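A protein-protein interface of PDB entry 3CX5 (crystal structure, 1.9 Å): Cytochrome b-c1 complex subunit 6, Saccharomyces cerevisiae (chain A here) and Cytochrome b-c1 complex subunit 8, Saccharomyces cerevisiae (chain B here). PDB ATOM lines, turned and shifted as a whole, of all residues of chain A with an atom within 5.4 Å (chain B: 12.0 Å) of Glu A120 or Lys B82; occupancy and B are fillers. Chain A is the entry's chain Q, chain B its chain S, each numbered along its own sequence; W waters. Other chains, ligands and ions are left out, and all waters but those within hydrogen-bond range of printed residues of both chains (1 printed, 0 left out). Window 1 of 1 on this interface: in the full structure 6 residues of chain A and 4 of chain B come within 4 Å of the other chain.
Cys A100 touches just one residue of chain B: Lys B82 (3.7 Å).
No residue of chain B comes within 4 Å of Arg A103.
No residue of chain B comes within 4 Å of Val A104.
Of the printed residues of chain B, His A118 touches Arg B85 and Glu B89.
No residue of chain B comes within 4 Å of Lys A119.
Glu A120 touches one residue of chain B.
No residue of chain B comes within 4 Å of Cys A122.
Glu A124 touches just these residues of chain B: Ser B81 (3.5 Å) and Lys B82 (2.8 Å).
Printed residues of chain A within 4 Å of Ser B81: Glu A124 (3.5 Å).
Printed residues of chain A within 4 Å of Arg B85: His A118.
Of the printed residues of chain A, Glu B89 touches His A118 (3.2 Å).
Of the 12 printed residues of chain A, 6 touch a printed residue of chain B.
Hydrophobic or aromatic side chains of chain A that line the printed part of chain B: His A118.
OE2 of Glu B89 is in hydrogen-bond range of NE2 of His A118.
The side-chain carboxylate of Glu A125 is in salt-bridge range of the side-chain amino group of Lys B82.
N of Lys B82 is in hydrogen-bond range of OE2 of Glu A124 (2.8 Å).
NZ of Lys B82 is in salt-bridge range of OE2 of Glu A120 (3.2 Å).
SG of Cys A100 is in hydrogen-bond range of NZ of Lys B82, 3.7 Å away.
The backbone carbonyl oxygen (O) of Asp A121 lies within hydrogen-bond range of the side-chain amino group (NZ) of Lys B82 (2.9 Å).
Arg B85 touches His A118 (NH1 to CD2, 3.2 Å).
Glu A124 touches Ser B81.
The side-chain carboxylate of Glu A120 lies within hydrogen-bond range of the side-chain amide nitrogen of Gln A107, at 3.2 Å.
O of Phe B78 sits at hydrogen-bond distance from OG of Ser B81 (2.6 Å).
OG of Ser B81 sits at hydrogen-bond distance from N of Gly B84 (3.5 Å).
The guanidinium group (NH1) of Arg B85 lies within salt-bridge range of the side-chain carboxylate (OE2) of Glu B89 (3.3 Å).
The guanidinium group (NH2) of Arg B85 lies within salt-bridge range of the side-chain carboxylate (OE2) of Glu B86, 3.0 Å away.
OE2 of Glu A120 lies within salt-bridge range of NH1 of Arg A103 (3.0 Å).
Water W1 lies within hydrogen-bond range of the side-chain carboxylate (OE1) of Glu A124, the backbone NH (N) of Ala B83 and the backbone NH (N) of Lys B82.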
ATOM      1  N   CYS A 100      35.380   9.423 -23.191  1.00  0.00           N
ATOM      2  CA  CYS A 100      34.091   9.011 -22.645  1.00  0.00           C
ATOM      3  C   CYS A 100      34.262   7.715 -21.862  1.00  0.00           C
ATOM      4  O   CYS A 100      33.705   7.559 -20.779  1.00  0.00           O
ATOM      5  CB  CYS A 100      33.061   8.805 -23.767  1.00  0.00           C
ATOM      6  SG  CYS A 100      31.460   8.118 -23.214  1.00  0.00           S
ATOM      7  N   ARG A 103      35.820   8.363 -18.473  1.00  0.00           N
ATOM      8  CA  ARG A 103      34.821   9.007 -17.625  1.00  0.00           C
ATOM      9  C   ARG A 103      33.824   7.984 -17.076  1.00  0.00           C
ATOM     10  O   ARG A 103      33.419   8.063 -15.916  1.00  0.00           O
ATOM     11  CB  ARG A 103      34.091  10.097 -18.419  1.00  0.00           C
ATOM     12  CG  ARG A 103      33.065  10.884 -17.625  1.00  0.00           C
ATOM     13  CD  ARG A 103      32.597  12.126 -18.382  1.00  0.00           C
ATOM     14  NE  ARG A 103      31.863  11.808 -19.606  1.00  0.00           N
ATOM     15  CZ  ARG A 103      32.335  12.000 -20.836  1.00  0.00           C
ATOM     16  NH1 ARG A 103      31.593  11.681 -21.889  1.00  0.00           N
ATOM     17  NH2 ARG A 103      33.549  12.506 -21.014  1.00  0.00           N
ATOM     18  N   VAL A 104      33.445   7.019 -17.911  1.00  0.00           N
ATOM     19  CA  VAL A 104      32.508   5.974 -17.513  1.00  0.00           C
ATOM     20  C   VAL A 104      33.177   5.004 -16.539  1.00  0.00           C
ATOM     21  O   VAL A 104      32.556   4.554 -15.574  1.00  0.00           O
ATOM     22  CB  VAL A 104      31.964   5.209 -18.746  1.00  0.00           C
ATOM     23  CG1 VAL A 104      31.180   3.975 -18.316  1.00  0.00           C
ATOM     24  CG2 VAL A 104      31.071   6.130 -19.568  1.00  0.00           C
ATOM     25  N   GLN A 107      32.948   6.525 -13.146  1.00  0.00           N
ATOM     26  CA  GLN A 107      31.591   6.510 -12.602  1.00  0.00           C
ATOM     27  C   GLN A 107      31.252   5.154 -11.991  1.00  0.00           C
ATOM     28  O   GLN A 107      30.562   5.077 -10.974  1.00  0.00           O
ATOM     29  CB  GLN A 107      30.568   6.821 -13.696  1.00  0.00           C
ATOM     30  CG  GLN A 107      30.638   8.222 -14.270  1.00  0.00           C
ATOM     31  CD  GLN A 107      29.632   8.439 -15.391  1.00  0.00           C
ATOM     32  OE1 GLN A 107      28.743   7.614 -15.615  1.00  0.00           O
ATOM     33  NE2 GLN A 107      29.771   9.553 -16.103  1.00  0.00           N
ATOM     34  N   TYR A 113      26.695   2.688  -7.810  1.00  0.00           N
ATOM     35  CA  TYR A 113      26.598   2.863  -9.254  1.00  0.00           C
ATOM     36  C   TYR A 113      25.415   2.078  -9.818  1.00  0.00           C
ATOM     37  O   TYR A 113      24.751   2.531 -10.754  1.00  0.00           O
ATOM     38  CB  TYR A 113      27.899   2.420  -9.938  1.00  0.00           C
ATOM     39  CG  TYR A 113      27.832   2.417 -11.451  1.00  0.00           C
ATOM     40  CD1 TYR A 113      27.716   1.219 -12.157  1.00  0.00           C
ATOM     41  CD2 TYR A 113      27.861   3.607 -12.176  1.00  0.00           C
ATOM     42  CE1 TYR A 113      27.628   1.206 -13.546  1.00  0.00           C
ATOM     43  CE2 TYR A 113      27.775   3.606 -13.568  1.00  0.00           C
ATOM     44  CZ  TYR A 113      27.657   2.403 -14.245  1.00  0.00           C
ATOM     45  OH  TYR A 113      27.561   2.391 -15.617  1.00  0.00           O
ATOM     46  N   HIS A 118      20.471   6.693 -14.544  1.00  0.00           N
ATOM     47  CA  HIS A 118      20.946   7.668 -15.524  1.00  0.00           C
ATOM     48  C   HIS A 118      22.426   7.411 -15.805  1.00  0.00           C
ATOM     49  O   HIS A 118      23.249   8.329 -15.769  1.00  0.00           O
ATOM     50  CB  HIS A 118      20.751   9.102 -15.011  1.00  0.00           C
ATOM     51  CG  HIS A 118      19.354   9.621 -15.168  1.00  0.00           C
ATOM     52  ND1 HIS A 118      18.710  10.334 -14.180  1.00  0.00           N
ATOM     53  CD2 HIS A 118      18.483   9.542 -16.203  1.00  0.00           C
ATOM     54  CE1 HIS A 118      17.503  10.674 -14.600  1.00  0.00           C
ATOM     55  NE2 HIS A 118      17.341  10.204 -15.824  1.00  0.00           N
ATOM     56  N   LYS A 119      22.754   6.149 -16.068  1.00  0.00           N
ATOM     57  CA  LYS A 119      24.125   5.737 -16.353  1.00  0.00           C
ATOM     58  C   LYS A 119      24.544   6.064 -17.785  1.00  0.00           C
ATOM     59  O   LYS A 119      23.874   5.676 -18.743  1.00  0.00           O
ATOM     60  CB  LYS A 119      24.285   4.238 -16.071  1.00  0.00           C
ATOM     61  CG  LYS A 119      24.229   3.889 -14.583  1.00  0.00           C
ATOM     62  CD  LYS A 119      24.095   2.390 -14.338  1.00  0.00           C
ATOM     63  CE  LYS A 119      22.646   1.927 -14.437  1.00  0.00           C
ATOM     64  NZ  LYS A 119      21.796   2.492 -13.345  1.00  0.00           N
ATOM     65  N   GLU A 120      25.645   6.798 -17.920  1.00  0.00           N
ATOM     66  CA  GLU A 120      26.159   7.186 -19.229  1.00  0.00           C
ATOM     67  C   GLU A 120      26.912   6.053 -19.923  1.00  0.00           C
ATOM     68  O   GLU A 120      27.605   5.262 -19.280  1.00  0.00           O
ATOM     69  CB  GLU A 120      27.087   8.403 -19.102  1.00  0.00           C
ATOM     70  CG  GLU A 120      27.708   8.859 -20.430  1.00  0.00           C
ATOM     71  CD  GLU A 120      28.766   9.951 -20.280  1.00  0.00           C
ATOM     72  OE1 GLU A 120      29.539   9.930 -19.298  1.00  0.00           O
ATOM     73  OE2 GLU A 120      28.841  10.827 -21.167  1.00  0.00           O
ATOM     74  N   ASP A 121      26.745   5.967 -21.237  1.00  0.00           N
ATOM     75  CA  ASP A 121      27.439   4.967 -22.037  1.00  0.00           C
ATOM     76  C   ASP A 121      28.116   5.706 -23.183  1.00  0.00           C
ATOM     77  O   ASP A 121      27.836   6.884 -23.415  1.00  0.00           O
ATOM     78  CB  ASP A 121      26.475   3.889 -22.555  1.00  0.00           C
ATOM     79  CG  ASP A 121      25.376   4.450 -23.441  1.00  0.00           C
ATOM     80  OD1 ASP A 121      24.226   4.559 -22.964  1.00  0.00           O
ATOM     81  OD2 ASP A 121      25.659   4.768 -24.615  1.00  0.00           O
ATOM     82  N   CYS A 122      28.986   5.016 -23.912  1.00  0.00           N
ATOM     83  CA  CYS A 122      29.704   5.646 -25.010  1.00  0.00           C
ATOM     84  C   CYS A 122      29.303   5.155 -26.400  1.00  0.00           C
ATOM     85  O   CYS A 122      30.120   5.132 -27.325  1.00  0.00           O
ATOM     86  CB  CYS A 122      31.215   5.502 -24.792  1.00  0.00           C
ATOM     87  SG  CYS A 122      31.772   6.103 -23.158  1.00  0.00           S
ATOM     88  N   GLU A 124      27.177   6.637 -28.521  1.00  0.00           N
ATOM     89  CA  GLU A 124      27.181   7.785 -29.424  1.00  0.00           C
ATOM     90  C   GLU A 124      28.585   8.106 -29.941  1.00  0.00           C
ATOM     91  O   GLU A 124      28.782   8.300 -31.143  1.00  0.00           O
ATOM     92  CB  GLU A 124      26.568   8.994 -28.724  1.00  0.00           C
ATOM     93  CG  GLU A 124      26.311  10.180 -29.626  1.00  0.00           C
ATOM     94  CD  GLU A 124      25.607  11.315 -28.898  1.00  0.00           C
ATOM     95  OE1 GLU A 124      26.253  12.358 -28.662  1.00  0.00           O
ATOM     96  OE2 GLU A 124      24.410  11.159 -28.557  1.00  0.00           O
ATOM     97  N   GLU A 125      29.563   8.100 -29.042  1.00  0.00           N
ATOM     98  CA  GLU A 125      30.951   8.377 -29.411  1.00  0.00           C
ATOM     99  C   GLU A 125      31.482   7.276 -30.316  1.00  0.00           C
ATOM    100  O   GLU A 125      32.171   7.554 -31.299  1.00  0.00           O
ATOM    101  CB  GLU A 125      31.835   8.497 -28.165  1.00  0.00           C
ATOM    102  CG  GLU A 125      31.587   9.740 -27.321  1.00  0.00           C
ATOM    103  CD  GLU A 125      30.388   9.621 -26.390  1.00  0.00           C
ATOM    104  OE1 GLU A 125      29.688   8.584 -26.416  1.00  0.00           O
ATOM    105  OE2 GLU A 125      30.149  10.576 -25.619  1.00  0.00           O
ATOM    106  N   GLU B  74      15.521  18.257 -37.112  1.00  0.00           N
ATOM    107  CA  GLU B  74      16.774  18.589 -36.427  1.00  0.00           C
ATOM    108  C   GLU B  74      16.569  18.652 -34.919  1.00  0.00           C
ATOM    109  O   GLU B  74      17.433  18.233 -34.147  1.00  0.00           O
ATOM    110  CB  GLU B  74      17.326  19.919 -36.938  1.00  0.00           C
ATOM    111  CG  GLU B  74      17.820  19.850 -38.378  1.00  0.00           C
ATOM    112  CD  GLU B  74      17.979  21.218 -39.031  1.00  0.00           C
ATOM    113  OE1 GLU B  74      18.613  21.282 -40.109  1.00  0.00           O
ATOM    114  OE2 GLU B  74      17.461  22.221 -38.490  1.00  0.00           O
ATOM    115  N   TYR B  75      15.417  19.166 -34.502  1.00  0.00           N
ATOM    116  CA  TYR B  75      15.110  19.250 -33.086  1.00  0.00           C
ATOM    117  C   TYR B  75      14.950  17.839 -32.508  1.00  0.00           C
ATOM    118  O   TYR B  75      15.381  17.572 -31.386  1.00  0.00           O
ATOM    119  CB  TYR B  75      13.843  20.075 -32.864  1.00  0.00           C
ATOM    120  CG  TYR B  75      13.477  20.257 -31.409  1.00  0.00           C
ATOM    121  CD1 TYR B  75      14.423  20.693 -30.475  1.00  0.00           C
ATOM    122  CD2 TYR B  75      12.184  19.995 -30.964  1.00  0.00           C
ATOM    123  CE1 TYR B  75      14.084  20.862 -29.131  1.00  0.00           C
ATOM    124  CE2 TYR B  75      11.834  20.161 -29.627  1.00  0.00           C
ATOM    125  CZ  TYR B  75      12.788  20.594 -28.719  1.00  0.00           C
ATOM    126  OH  TYR B  75      12.431  20.756 -27.405  1.00  0.00           O
ATOM    127  N   ASN B  76      14.356  16.937 -33.289  1.00  0.00           N
ATOM    128  CA  ASN B  76      14.163  15.548 -32.864  1.00  0.00           C
ATOM    129  C   ASN B  76      15.515  14.848 -32.696  1.00  0.00           C
ATOM    130  O   ASN B  76      15.729  14.121 -31.724  1.00  0.00           O
ATOM    131  CB  ASN B  76      13.293  14.789 -33.880  1.00  0.00           C
ATOM    132  CG  ASN B  76      13.167  13.310 -33.558  1.00  0.00           C
ATOM    133  OD1 ASN B  76      13.919  12.485 -34.088  1.00  0.00           O
ATOM    134  ND2 ASN B  76      12.214  12.963 -32.690  1.00  0.00           N
ATOM    135  N   GLU B  77      16.414  15.066 -33.654  1.00  0.00           N
ATOM    136  CA  GLU B  77      17.754  14.486 -33.622  1.00  0.00           C
ATOM    137  C   GLU B  77      18.521  14.955 -32.376  1.00  0.00           C
ATOM    138  O   GLU B  77      19.284  14.194 -31.781  1.00  0.00           O
ATOM    139  CB  GLU B  77      18.527  14.868 -34.888  1.00  0.00           C
ATOM    140  CG  GLU B  77      19.967  14.352 -34.922  1.00  0.00           C
ATOM    141  CD  GLU B  77      20.695  14.678 -36.221  1.00  0.00           C
ATOM    142  OE1 GLU B  77      20.550  15.815 -36.730  1.00  0.00           O
ATOM    143  OE2 GLU B  77      21.424  13.794 -36.729  1.00  0.00           O
ATOM    144  N   PHE B  78      18.301  16.205 -31.982  1.00  0.00           N
ATOM    145  CA  PHE B  78      18.949  16.764 -30.802  1.00  0.00           C
ATOM    146  C   PHE B  78      18.365  16.157 -29.526  1.00  0.00           C
ATOM    147  O   PHE B  78      19.105  15.773 -28.614  1.00  0.00           O
ATOM    148  CB  PHE B  78      18.777  18.286 -30.775  1.00  0.00           C
ATOM    149  CG  PHE B  78      19.092  18.904 -29.448  1.00  0.00           C
ATOM    150  CD1 PHE B  78      20.414  19.051 -29.029  1.00  0.00           C
ATOM    151  CD2 PHE B  78      18.065  19.303 -28.592  1.00  0.00           C
ATOM    152  CE1 PHE B  78      20.710  19.584 -27.774  1.00  0.00           C
ATOM    153  CE2 PHE B  78      18.352  19.838 -27.334  1.00  0.00           C
ATOM    154  CZ  PHE B  78      19.678  19.976 -26.926  1.00  0.00           C
ATOM    155  N   LEU B  79      17.036  16.090 -29.462  1.00  0.00           N
ATOM    156  CA  LEU B  79      16.347  15.536 -28.302  1.00  0.00           C
ATOM    157  C   LEU B  79      16.761  14.108 -27.954  1.00  0.00           C
ATOM    158  O   LEU B  79      16.766  13.729 -26.783  1.00  0.00           O
ATOM    159  CB  LEU B  79      14.833  15.591 -28.502  1.00  0.00           C
ATOM    160  CG  LEU B  79      14.182  16.964 -28.350  1.00  0.00           C
ATOM    161  CD1 LEU B  79      12.688  16.833 -28.556  1.00  0.00           C
ATOM    162  CD2 LEU B  79      14.473  17.524 -26.961  1.00  0.00           C
ATOM    163  N   TYR B  80      17.127  13.328 -28.968  1.00  0.00           N
ATOM    164  CA  TYR B  80      17.527  11.948 -28.746  1.00  0.00           C
ATOM    165  C   TYR B  80      19.027  11.708 -28.711  1.00  0.00           C
ATOM    166  O   TYR B  80      19.482  10.564 -28.707  1.00  0.00           O
ATOM    167  CB  TYR B  80      16.816  11.019 -29.733  1.00  0.00           C
ATOM    168  CG  TYR B  80      15.367  10.818 -29.351  1.00  0.00           C
ATOM    169  CD1 TYR B  80      14.379  11.695 -29.799  1.00  0.00           C
ATOM    170  CD2 TYR B  80      14.996   9.802 -28.465  1.00  0.00           C
ATOM    171  CE1 TYR B  80      13.062  11.574 -29.368  1.00  0.00           C
ATOM    172  CE2 TYR B  80      13.682   9.670 -28.031  1.00  0.00           C
ATOM    173  CZ  TYR B  80      12.723  10.561 -28.482  1.00  0.00           C
ATOM    174  OH  TYR B  80      11.428  10.451 -28.034  1.00  0.00           O
ATOM    175  N   SER B  81      19.794  12.792 -28.691  1.00  0.00           N
ATOM    176  CA  SER B  81      21.244  12.693 -28.597  1.00  0.00           C
ATOM    177  C   SER B  81      21.560  12.839 -27.106  1.00  0.00           C
ATOM    178  O   SER B  81      20.690  13.234 -26.319  1.00  0.00           O
ATOM    179  CB  SER B  81      21.920  13.815 -29.390  1.00  0.00           C
ATOM    180  OG  SER B  81      21.644  15.081 -28.815  1.00  0.00           O
ATOM    181  N   LYS B  82      22.794  12.525 -26.721  1.00  0.00           N
ATOM    182  CA  LYS B  82      23.214  12.631 -25.325  1.00  0.00           C
ATOM    183  C   LYS B  82      23.016  14.055 -24.783  1.00  0.00           C
ATOM    184  O   LYS B  82      22.508  14.241 -23.676  1.00  0.00           O
ATOM    185  CB  LYS B  82      24.681  12.197 -25.184  1.00  0.00           C
ATOM    186  CG  LYS B  82      25.136  11.994 -23.745  1.00  0.00           C
ATOM    187  CD  LYS B  82      26.586  11.533 -23.659  1.00  0.00           C
ATOM    188  CE  LYS B  82      26.771  10.158 -24.277  1.00  0.00           C
ATOM    189  NZ  LYS B  82      28.163   9.659 -24.093  1.00  0.00           N
ATOM    190  N   ALA B  83      23.361  15.051 -25.597  1.00  0.00           N
ATOM    191  CA  ALA B  83      23.232  16.459 -25.218  1.00  0.00           C
ATOM    192  C   ALA B  83      21.789  16.934 -25.034  1.00  0.00           C
ATOM    193  O   ALA B  83      21.542  17.928 -24.347  1.00  0.00           O
ATOM    194  CB  ALA B  83      23.930  17.333 -26.240  1.00  0.00           C
ATOM    195  N   GLY B  84      20.840  16.231 -25.647  1.00  0.00           N
ATOM    196  CA  GLY B  84      19.450  16.625 -25.533  1.00  0.00           C
ATOM    197  C   GLY B  84      18.624  15.862 -24.517  1.00  0.00           C
ATOM    198  O   GLY B  84      17.440  16.161 -24.344  1.00  0.00           O
ATOM    199  N   ARG B  85      19.237  14.901 -23.826  1.00  0.00           N
ATOM    200  CA  ARG B  85      18.516  14.093 -22.838  1.00  0.00           C
ATOM    201  C   ARG B  85      17.795  14.901 -21.760  1.00  0.00           C
ATOM    202  O   ARG B  85      16.695  14.538 -21.341  1.00  0.00           O
ATOM    203  CB  ARG B  85      19.441  13.056 -22.188  1.00  0.00           C
ATOM    204  CG  ARG B  85      20.642  13.635 -21.461  1.00  0.00           C
ATOM    205  CD  ARG B  85      21.420  12.559 -20.707  1.00  0.00           C
ATOM    206  NE  ARG B  85      20.688  12.061 -19.542  1.00  0.00           N
ATOM    207  CZ  ARG B  85      20.665  12.664 -18.354  1.00  0.00           C
ATOM    208  NH1 ARG B  85      19.969  12.137 -17.354  1.00  0.00           N
ATOM    209  NH2 ARG B  85      21.341  13.791 -18.162  1.00  0.00           N
ATOM    210  N   GLU B  86      18.404  16.004 -21.334  1.00  0.00           N
ATOM    211  CA  GLU B  86      17.822  16.867 -20.308  1.00  0.00           C
ATOM    212  C   GLU B  86      16.498  17.443 -20.800  1.00  0.00           C
ATOM    213  O   GLU B  86      15.463  17.291 -20.150  1.00  0.00           O
ATOM    214  CB  GLU B  86      18.784  18.015 -19.979  1.00  0.00           C
ATOM    215  CG  GLU B  86      18.822  18.414 -18.511  1.00  0.00           C
ATOM    216  CD  GLU B  86      19.866  17.639 -17.715  1.00  0.00           C
ATOM    217  OE1 GLU B  86      20.662  18.289 -17.002  1.00  0.00           O
ATOM    218  OE2 GLU B  86      19.898  16.390 -17.802  1.00  0.00           O
ATOM    219  N   GLU B  87      16.539  18.083 -21.965  1.00  0.00           N
ATOM    220  CA  GLU B  87      15.348  18.683 -22.557  1.00  0.00           C
ATOM    221  C   GLU B  87      14.308  17.644 -22.980  1.00  0.00           C
ATOM    222  O   GLU B  87      13.111  17.929 -22.978  1.00  0.00           O
ATOM    223  CB  GLU B  87      15.731  19.570 -23.743  1.00  0.00           C
ATOM    224  CG  GLU B  87      14.539  20.244 -24.401  1.00  0.00           C
ATOM    225  CD  GLU B  87      14.912  21.454 -25.232  1.00  0.00           C
ATOM    226  OE1 GLU B  87      16.116  21.666 -25.495  1.00  0.00           O
ATOM    227  OE2 GLU B  87      13.991  22.207 -25.616  1.00  0.00           O
ATOM    228  N   LEU B  88      14.770  16.446 -23.334  1.00  0.00           N
ATOM    229  CA  LEU B  88      13.880  15.363 -23.747  1.00  0.00           C
ATOM    230  C   LEU B  88      12.987  14.972 -22.575  1.00  0.00           C
ATOM    231  O   LEU B  88      11.771  14.854 -22.727  1.00  0.00           O
ATOM    232  CB  LEU B  88      14.697  14.158 -24.237  1.00  0.00           C
ATOM    233  CG  LEU B  88      14.022  12.916 -24.846  1.00  0.00           C
ATOM    234  CD1 LEU B  88      13.558  11.953 -23.767  1.00  0.00           C
ATOM    235  CD2 LEU B  88      12.872  13.318 -25.760  1.00  0.00           C
ATOM    236  N   GLU B  89      13.593  14.805 -21.403  1.00  0.00           N
ATOM    237  CA  GLU B  89      12.861  14.443 -20.191  1.00  0.00           C
ATOM    238  C   GLU B  89      11.827  15.509 -19.839  1.00  0.00           C
ATOM    239  O   GLU B  89      10.731  15.198 -19.373  1.00  0.00           O
ATOM    240  CB  GLU B  89      13.833  14.259 -19.021  1.00  0.00           C
ATOM    241  CG  GLU B  89      14.732  13.031 -19.150  1.00  0.00           C
ATOM    242  CD  GLU B  89      15.797  12.937 -18.062  1.00  0.00           C
ATOM    243  OE1 GLU B  89      15.630  13.555 -16.986  1.00  0.00           O
ATOM    244  OE2 GLU B  89      16.808  12.235 -18.291  1.00  0.00           O
ATOM    245  N   ARG B  90      12.178  16.762 -20.108  1.00  0.00           N
ATOM    246  CA  ARG B  90      11.317  17.902 -19.825  1.00  0.00           C
ATOM    247  C   ARG B  90      10.084  17.980 -20.736  1.00  0.00           C
ATOM    248  O   ARG B  90       8.957  18.089 -20.252  1.00  0.00           O
ATOM    249  CB  ARG B  90      12.134  19.187 -19.951  1.00  0.00           C
ATOM    250  CG  ARG B  90      11.470  20.433 -19.405  1.00  0.00           C
ATOM    251  CD  ARG B  90      12.247  21.673 -19.831  1.00  0.00           C
ATOM    252  NE  ARG B  90      13.679  21.549 -19.556  1.00  0.00           N
ATOM    253  CZ  ARG B  90      14.640  21.811 -20.440  1.00  0.00           C
ATOM    254  NH1 ARG B  90      15.914  21.668 -20.097  1.00  0.00           N
ATOM    255  NH2 ARG B  90      14.330  22.214 -21.668  1.00  0.00           N
HETATM  256  O   HOH W   1      25.054  14.608 -27.845  1.00  0.00           O
